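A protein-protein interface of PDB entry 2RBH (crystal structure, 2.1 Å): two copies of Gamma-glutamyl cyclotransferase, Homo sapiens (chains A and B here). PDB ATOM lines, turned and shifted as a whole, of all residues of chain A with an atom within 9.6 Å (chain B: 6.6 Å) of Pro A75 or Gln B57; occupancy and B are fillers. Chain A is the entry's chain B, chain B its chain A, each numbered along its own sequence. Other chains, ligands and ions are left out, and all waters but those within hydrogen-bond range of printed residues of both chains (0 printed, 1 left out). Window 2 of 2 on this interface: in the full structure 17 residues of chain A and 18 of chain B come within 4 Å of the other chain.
The side-chain amide nitrogen of Gln B57 sits at hydrogen-bond distance from the backbone carbonyl oxygen of Gln A73 (3.3 Å).
O of Gly B103 sits close to OE1 of Gln A73, 3.4 Å away.
The side-chain hydroxyl (OG1) of Thr B128 lies within hydrogen-bond range of the side-chain amide oxygen (OE1) of Gln A73.
ND2 of Asn B129 lies within hydrogen-bond range of O of Gln A73 (3.0 Å).
The side-chain amide nitrogen of Gln B57 sits at hydrogen-bond distance from the backbone carbonyl oxygen of Gly B103.
The backbone carbonyl oxygen (O) of Asn B129 is in hydrogen-bond range of the backbone NH (N) of Gln B57 (2.8 Å).
N of Lys A50 is in hydrogen-bond range of O of Phe A72.
Thr B128 touches Phe A72.
Pro A75 touches Gln B57.
Of the printed residues of chain B, Phe A72 touches Thr B128.
Of the printed residues of chain B, Gln A73 touches Gln B57, Gly B103, Thr B128 and Asn B129.
Ser A74 touches none of the printed residues of chain B.
Of chain B, only Gln B57 (3.7 Å) comes within 4 Å of Pro A75.
No residue of chain A comes within 4 Å of Ser B56.
Gln B57 touches just these residues of chain A: Gln A73 and Pro A75.
No residue of chain A comes within 4 Å of Gly B58.
Gly B103 touches just one residue of chain A: Gln A73 (3.4 Å).
Asn B129 touches one residue of chain A.
Tyr B130 touches none of the printed residues of chain A.
The nearest residue of chain B that does not touch Pro A75 is Ser B102 (4.5 Å).
The nearest residue of chain A that does not touch Gln B57 is Ser A74 (4.3 Å).
Of the 12 printed residues of chain A, 3 touch a printed residue of chain B.
Hydrophobic or aromatic side chains of chain A that line the printed part of chain B: Phe A72 and Pro A75.
Of the 14 printed residues of chain B, 4 touch a printed residue of chain A.
No position is printed for both chains.
Of the 6 pairs that touch across the chains among the printed residues, none has its exchanged pair printed and touching as well.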
ATOM      1  N   LEU A  46     -35.299   8.142  22.120  1.00  0.00           N
ATOM      2  CA  LEU A  46     -33.928   8.430  21.710  1.00  0.00           C
ATOM      3  C   LEU A  46     -33.079   8.574  22.982  1.00  0.00           C
ATOM      4  O   LEU A  46     -33.177   9.578  23.694  1.00  0.00           O
ATOM      5  CB  LEU A  46     -33.882   9.708  20.861  1.00  0.00           C
ATOM      6  CG  LEU A  46     -32.519  10.193  20.341  1.00  0.00           C
ATOM      7  CD1 LEU A  46     -31.807   9.121  19.517  1.00  0.00           C
ATOM      8  CD2 LEU A  46     -32.684  11.461  19.533  1.00  0.00           C
ATOM      9  N   GLN A  47     -32.279   7.550  23.269  1.00  0.00           N
ATOM     10  CA  GLN A  47     -31.472   7.501  24.493  1.00  0.00           C
ATOM     11  C   GLN A  47     -30.287   8.454  24.407  1.00  0.00           C
ATOM     12  O   GLN A  47     -29.759   8.672  23.314  1.00  0.00           O
ATOM     13  CB  GLN A  47     -30.985   6.067  24.751  1.00  0.00           C
ATOM     14  CG  GLN A  47     -30.553   5.772  26.206  1.00  0.00           C
ATOM     15  CD  GLN A  47     -31.536   6.323  27.266  1.00  0.00           C
ATOM     16  OE1 GLN A  47     -32.758   6.159  27.152  1.00  0.00           O
ATOM     17  NE2 GLN A  47     -30.992   6.984  28.301  1.00  0.00           N
ATOM     18  N   ASP A  48     -29.881   9.016  25.551  1.00  0.00           N
ATOM     19  CA  ASP A  48     -28.698   9.906  25.656  1.00  0.00           C
ATOM     20  C   ASP A  48     -28.717  11.186  24.803  1.00  0.00           C
ATOM     21  O   ASP A  48     -27.661  11.663  24.343  1.00  0.00           O
ATOM     22  CB  ASP A  48     -27.405   9.127  25.404  1.00  0.00           C
ATOM     23  CG  ASP A  48     -27.292   7.906  26.282  1.00  0.00           C
ATOM     24  OD1 ASP A  48     -27.567   8.016  27.495  1.00  0.00           O
ATOM     25  OD2 ASP A  48     -26.951   6.839  25.741  1.00  0.00           O
ATOM     26  N   PHE A  49     -29.920  11.729  24.604  1.00  0.00           N
ATOM     27  CA  PHE A  49     -30.125  13.050  24.015  1.00  0.00           C
ATOM     28  C   PHE A  49     -31.051  13.827  24.975  1.00  0.00           C
ATOM     29  O   PHE A  49     -31.921  13.236  25.625  1.00  0.00           O
ATOM     30  CB  PHE A  49     -30.809  12.945  22.645  1.00  0.00           C
ATOM     31  CG  PHE A  49     -29.874  12.704  21.475  1.00  0.00           C
ATOM     32  CD1 PHE A  49     -29.306  11.444  21.249  1.00  0.00           C
ATOM     33  CD2 PHE A  49     -29.621  13.726  20.548  1.00  0.00           C
ATOM     34  CE1 PHE A  49     -28.493  11.220  20.131  1.00  0.00           C
ATOM     35  CE2 PHE A  49     -28.798  13.513  19.428  1.00  0.00           C
ATOM     36  CZ  PHE A  49     -28.239  12.254  19.223  1.00  0.00           C
ATOM     37  N   LYS A  50     -30.858  15.144  25.056  1.00  0.00           N
ATOM     38  CA  LYS A  50     -31.702  16.026  25.863  1.00  0.00           C
ATOM     39  C   LYS A  50     -32.484  16.968  24.937  1.00  0.00           C
ATOM     40  O   LYS A  50     -31.969  17.391  23.893  1.00  0.00           O
ATOM     41  CB  LYS A  50     -30.837  16.830  26.842  1.00  0.00           C
ATOM     42  CG  LYS A  50     -31.619  17.819  27.731  1.00  0.00           C
ATOM     43  CD  LYS A  50     -30.723  18.455  28.801  1.00  0.00           C
ATOM     44  CE  LYS A  50     -31.536  19.060  29.965  1.00  0.00           C
ATOM     45  NZ  LYS A  50     -30.606  19.690  30.979  1.00  0.00           N
ATOM     46  N   PHE A  72     -29.689  17.604  21.713  1.00  0.00           N
ATOM     47  CA  PHE A  72     -28.239  17.414  21.702  1.00  0.00           C
ATOM     48  C   PHE A  72     -27.870  16.228  22.579  1.00  0.00           C
ATOM     49  O   PHE A  72     -28.620  15.873  23.498  1.00  0.00           O
ATOM     50  CB  PHE A  72     -27.512  18.695  22.169  1.00  0.00           C
ATOM     51  CG  PHE A  72     -27.815  19.099  23.588  1.00  0.00           C
ATOM     52  CD1 PHE A  72     -27.061  18.592  24.651  1.00  0.00           C
ATOM     53  CD2 PHE A  72     -28.826  20.025  23.862  1.00  0.00           C
ATOM     54  CE1 PHE A  72     -27.316  18.977  25.950  1.00  0.00           C
ATOM     55  CE2 PHE A  72     -29.085  20.422  25.170  1.00  0.00           C
ATOM     56  CZ  PHE A  72     -28.329  19.894  26.218  1.00  0.00           C
ATOM     57  N   GLN A  73     -26.701  15.641  22.317  1.00  0.00           N
ATOM     58  CA  GLN A  73     -26.249  14.456  23.054  1.00  0.00           C
ATOM     59  C   GLN A  73     -25.887  14.778  24.479  1.00  0.00           C
ATOM     60  O   GLN A  73     -25.157  15.737  24.756  1.00  0.00           O
ATOM     61  CB  GLN A  73     -25.068  13.783  22.346  1.00  0.00           C
ATOM     62  CG  GLN A  73     -25.450  13.227  20.993  1.00  0.00           C
ATOM     63  CD  GLN A  73     -24.279  13.152  20.066  1.00  0.00           C
ATOM     64  OE1 GLN A  73     -23.556  14.128  19.901  1.00  0.00           O
ATOM     65  NE2 GLN A  73     -24.070  11.984  19.458  1.00  0.00           N
ATOM     66  N   SER A  74     -26.393  13.945  25.381  1.00  0.00           N
ATOM     67  CA  SER A  74     -26.313  14.186  26.801  1.00  0.00           C
ATOM     68  C   SER A  74     -26.609  12.849  27.501  1.00  0.00           C
ATOM     69  O   SER A  74     -27.780  12.452  27.635  1.00  0.00           O
ATOM     70  CB  SER A  74     -27.330  15.274  27.184  1.00  0.00           C
ATOM     71  OG  SER A  74     -27.473  15.394  28.579  1.00  0.00           O
ATOM     72  N   PRO A  75     -25.545  12.107  27.871  1.00  0.00           N
ATOM     73  CA  PRO A  75     -25.705  10.794  28.508  1.00  0.00           C
ATOM     74  C   PRO A  75     -26.652  10.812  29.716  1.00  0.00           C
ATOM     75  O   PRO A  75     -26.570  11.708  30.555  1.00  0.00           O
ATOM     76  CB  PRO A  75     -24.273  10.444  28.923  1.00  0.00           C
ATOM     77  CG  PRO A  75     -23.439  11.095  27.838  1.00  0.00           C
ATOM     78  CD  PRO A  75     -24.118  12.425  27.637  1.00  0.00           C
ATOM     79  N   GLY A  76     -27.551   9.838  29.787  1.00  0.00           N
ATOM     80  CA  GLY A  76     -28.498   9.767  30.902  1.00  0.00           C
ATOM     81  C   GLY A  76     -29.801  10.515  30.659  1.00  0.00           C
ATOM     82  O   GLY A  76     -30.750  10.368  31.416  1.00  0.00           O
ATOM     83  N   ASP A  77     -29.844  11.333  29.613  1.00  0.00           N
ATOM     84  CA  ASP A  77     -31.080  12.015  29.233  1.00  0.00           C
ATOM     85  C   ASP A  77     -31.784  11.191  28.147  1.00  0.00           C
ATOM     86  O   ASP A  77     -31.170  10.301  27.536  1.00  0.00           O
ATOM     87  CB  ASP A  77     -30.780  13.448  28.776  1.00  0.00           C
ATOM     88  CG  ASP A  77     -30.542  14.401  29.951  1.00  0.00           C
ATOM     89  OD1 ASP A  77     -31.485  14.642  30.732  1.00  0.00           O
ATOM     90  OD2 ASP A  77     -29.412  14.903  30.115  1.00  0.00           O
ATOM     91  N   GLU A  78     -33.078  11.440  27.950  1.00  0.00           N
ATOM     92  CA  GLU A  78     -33.802  10.825  26.846  1.00  0.00           C
ATOM     93  C   GLU A  78     -34.757  11.822  26.200  1.00  0.00           C
ATOM     94  O   GLU A  78     -35.107  12.851  26.799  1.00  0.00           O
ATOM     95  CB  GLU A  78     -34.533   9.553  27.289  1.00  0.00           C
ATOM     96  CG  GLU A  78     -35.683   9.794  28.246  1.00  0.00           C
ATOM     97  CD  GLU A  78     -36.219   8.516  28.857  1.00  0.00           C
ATOM     98  OE1 GLU A  78     -35.431   7.568  29.081  1.00  0.00           O
ATOM     99  OE2 GLU A  78     -37.432   8.479  29.143  1.00  0.00           O
ATOM    100  N   ASN B  55     -13.485  19.488  22.882  1.00  0.00           N
ATOM    101  CA  ASN B  55     -13.546  18.350  23.777  1.00  0.00           C
ATOM    102  C   ASN B  55     -14.987  17.891  23.895  1.00  0.00           C
ATOM    103  O   ASN B  55     -15.788  18.526  24.557  1.00  0.00           O
ATOM    104  CB  ASN B  55     -12.988  18.760  25.135  1.00  0.00           C
ATOM    105  CG  ASN B  55     -11.548  19.196  25.056  1.00  0.00           C
ATOM    106  OD1 ASN B  55     -10.775  18.653  24.277  1.00  0.00           O
ATOM    107  ND2 ASN B  55     -11.178  20.170  25.861  1.00  0.00           N
ATOM    108  N   SER B  56     -15.337  16.809  23.212  1.00  0.00           N
ATOM    109  CA  SER B  56     -16.722  16.346  23.232  1.00  0.00           C
ATOM    110  C   SER B  56     -17.115  15.856  24.620  1.00  0.00           C
ATOM    111  O   SER B  56     -16.378  15.114  25.255  1.00  0.00           O
ATOM    112  CB  SER B  56     -16.937  15.255  22.204  1.00  0.00           C
ATOM    113  OG  SER B  56     -18.295  14.837  22.225  1.00  0.00           O
ATOM    114  N   GLN B  57     -18.280  16.293  25.091  1.00  0.00           N
ATOM    115  CA  GLN B  57     -18.743  15.998  26.444  1.00  0.00           C
ATOM    116  C   GLN B  57     -17.727  16.427  27.509  1.00  0.00           C
ATOM    117  O   GLN B  57     -17.641  15.821  28.573  1.00  0.00           O
ATOM    118  CB  GLN B  57     -19.106  14.507  26.600  1.00  0.00           C
ATOM    119  CG  GLN B  57     -20.069  13.932  25.546  1.00  0.00           C
ATOM    120  CD  GLN B  57     -21.478  14.557  25.569  1.00  0.00           C
ATOM    121  OE1 GLN B  57     -21.897  15.161  26.556  1.00  0.00           O
ATOM    122  NE2 GLN B  57     -22.203  14.412  24.464  1.00  0.00           N
ATOM    123  N   GLY B  58     -16.967  17.481  27.220  1.00  0.00           N
ATOM    124  CA  GLY B  58     -15.953  17.983  28.138  1.00  0.00           C
ATOM    125  C   GLY B  58     -14.697  17.136  28.281  1.00  0.00           C
ATOM    126  O   GLY B  58     -13.763  17.522  28.983  1.00  0.00           O
ATOM    127  N   LYS B  59     -14.659  15.982  27.625  1.00  0.00           N
ATOM    128  CA  LYS B  59     -13.524  15.069  27.742  1.00  0.00           C
ATOM    129  C   LYS B  59     -12.509  15.381  26.657  1.00  0.00           C
ATOM    130  O   LYS B  59     -12.876  15.510  25.482  1.00  0.00           O
ATOM    131  CB  LYS B  59     -13.979  13.612  27.577  1.00  0.00           C
ATOM    132  CG  LYS B  59     -15.040  13.149  28.553  1.00  0.00           C
ATOM    133  CD  LYS B  59     -15.679  11.855  28.085  1.00  0.00           C
ATOM    134  CE  LYS B  59     -16.827  11.462  29.009  1.00  0.00           C
ATOM    135  NZ  LYS B  59     -18.090  11.243  28.233  1.00  0.00           N
ATOM    136  N   THR B  60     -11.238  15.475  27.040  1.00  0.00           N
ATOM    137  CA  THR B  60     -10.159  15.617  26.061  1.00  0.00           C
ATOM    138  C   THR B  60      -9.806  14.242  25.499  1.00  0.00           C
ATOM    139  O   THR B  60      -9.618  13.289  26.264  1.00  0.00           O
ATOM    140  CB  THR B  60      -8.905  16.273  26.677  1.00  0.00           C
ATOM    141  OG1 THR B  60      -9.264  17.515  27.291  1.00  0.00           O
ATOM    142  CG2 THR B  60      -7.833  16.533  25.612  1.00  0.00           C
ATOM    143  N   SER B 102     -21.258   6.701  22.306  1.00  0.00           N
ATOM    144  CA  SER B 102     -20.798   7.384  23.507  1.00  0.00           C
ATOM    145  C   SER B 102     -21.179   8.869  23.516  1.00  0.00           C
ATOM    146  O   SER B 102     -20.854   9.601  24.452  1.00  0.00           O
ATOM    147  CB  SER B 102     -19.280   7.220  23.660  1.00  0.00           C
ATOM    148  OG  SER B 102     -18.657   7.148  22.382  1.00  0.00           O
ATOM    149  N   GLY B 103     -21.858   9.306  22.458  1.00  0.00           N
ATOM    150  CA  GLY B 103     -22.329  10.683  22.344  1.00  0.00           C
ATOM    151  C   GLY B 103     -21.264  11.684  21.941  1.00  0.00           C
ATOM    152  O   GLY B 103     -21.412  12.886  22.199  1.00  0.00           O
ATOM    153  N   MET B 104     -20.195  11.189  21.311  1.00  0.00           N
ATOM    154  CA  MET B 104     -19.077  12.037  20.891  1.00  0.00           C
ATOM    155  C   MET B 104     -19.483  12.845  19.672  1.00  0.00           C
ATOM    156  O   MET B 104     -19.374  14.071  19.658  1.00  0.00           O
ATOM    157  CB  MET B 104     -17.831  11.195  20.594  1.00  0.00           C
ATOM    158  CG  MET B 104     -16.523  11.992  20.532  1.00  0.00           C
ATOM    159  SD  MET B 104     -15.027  10.995  20.286  1.00  0.00           S
ATOM    160  CE  MET B 104     -15.082   9.972  21.758  1.00  0.00           C
ATOM    161  N   MET B 127     -20.052  17.167  16.398  1.00  0.00           N
ATOM    162  CA  MET B 127     -20.298  17.109  17.839  1.00  0.00           C
ATOM    163  C   MET B 127     -21.468  18.009  18.200  1.00  0.00           C
ATOM    164  O   MET B 127     -21.589  19.115  17.648  1.00  0.00           O
ATOM    165  CB  MET B 127     -19.072  17.578  18.613  1.00  0.00           C
ATOM    166  CG  MET B 127     -17.774  16.874  18.290  1.00  0.00           C
ATOM    167  SD  MET B 127     -16.551  17.403  19.510  1.00  0.00           S
ATOM    168  CE  MET B 127     -15.722  18.724  18.676  1.00  0.00           C
ATOM    169  N   THR B 128     -22.334  17.544  19.108  1.00  0.00           N
ATOM    170  CA  THR B 128     -23.540  18.303  19.468  1.00  0.00           C
ATOM    171  C   THR B 128     -23.419  18.891  20.870  1.00  0.00           C
ATOM    172  O   THR B 128     -24.158  19.813  21.230  1.00  0.00           O
ATOM    173  CB  THR B 128     -24.853  17.468  19.355  1.00  0.00           C
ATOM    174  OG1 THR B 128     -24.814  16.354  20.254  1.00  0.00           O
ATOM    175  CG2 THR B 128     -25.076  16.974  17.941  1.00  0.00           C
ATOM    176  N   ASN B 129     -22.457  18.378  21.634  1.00  0.00           N
ATOM    177  CA  ASN B 129     -22.232  18.796  23.004  1.00  0.00           C
ATOM    178  C   ASN B 129     -20.743  18.780  23.302  1.00  0.00           C
ATOM    179  O   ASN B 129     -20.162  17.717  23.573  1.00  0.00           O
ATOM    180  CB  ASN B 129     -22.995  17.877  23.974  1.00  0.00           C
ATOM    181  CG  ASN B 129     -23.082  18.448  25.380  1.00  0.00           C
ATOM    182  OD1 ASN B 129     -22.884  19.646  25.587  1.00  0.00           O
ATOM    183  ND2 ASN B 129     -23.406  17.593  26.352  1.00  0.00           N
ATOM    184  N   TYR B 130     -20.115  19.956  23.234  1.00  0.00           N
ATOM    185  CA  TYR B 130     -18.670  20.034  23.388  1.00  0.00           C
ATOM    186  C   TYR B 130     -18.196  21.390  23.914  1.00  0.00           C
ATOM    187  O   TYR B 130     -18.921  22.388  23.832  1.00  0.00           O
ATOM    188  CB  TYR B 130     -17.962  19.693  22.059  1.00  0.00           C
ATOM    189  CG  TYR B 130     -18.003  20.797  21.012  1.00  0.00           C
ATOM    190  CD1 TYR B 130     -19.101  20.945  20.164  1.00  0.00           C
ATOM    191  CD2 TYR B 130     -16.925  21.681  20.863  1.00  0.00           C
ATOM    192  CE1 TYR B 130     -19.144  21.953  19.212  1.00  0.00           C
ATOM    193  CE2 TYR B 130     -16.947  22.692  19.906  1.00  0.00           C
ATOM    194  CZ  TYR B 130     -18.060  22.826  19.087  1.00  0.00           C
ATOM    195  OH  TYR B 130     -18.075  23.815  18.137  1.00  0.00           O
ATOM    196  N   GLU B 131     -16.977  21.401  24.438  1.00  0.00           N
ATOM    197  CA  GLU B 131     -16.264  22.646  24.759  1.00  0.00           C
ATOM    198  C   GLU B 131     -15.145  22.912  23.757  1.00  0.00           C
ATOM    199  O   GLU B 131     -14.330  22.039  23.474  1.00  0.00           O
ATOM    200  CB  GLU B 131     -15.662  22.609  26.168  1.00  0.00           C
ATOM    201  CG  GLU B 131     -16.688  22.681  27.289  1.00  0.00           C
ATOM    202  CD  GLU B 131     -16.277  21.887  28.526  1.00  0.00           C
ATOM    203  OE1 GLU B 131     -15.113  21.426  28.595  1.00  0.00           O
ATOM    204  OE2 GLU B 131     -17.124  21.724  29.435  1.00  0.00           O
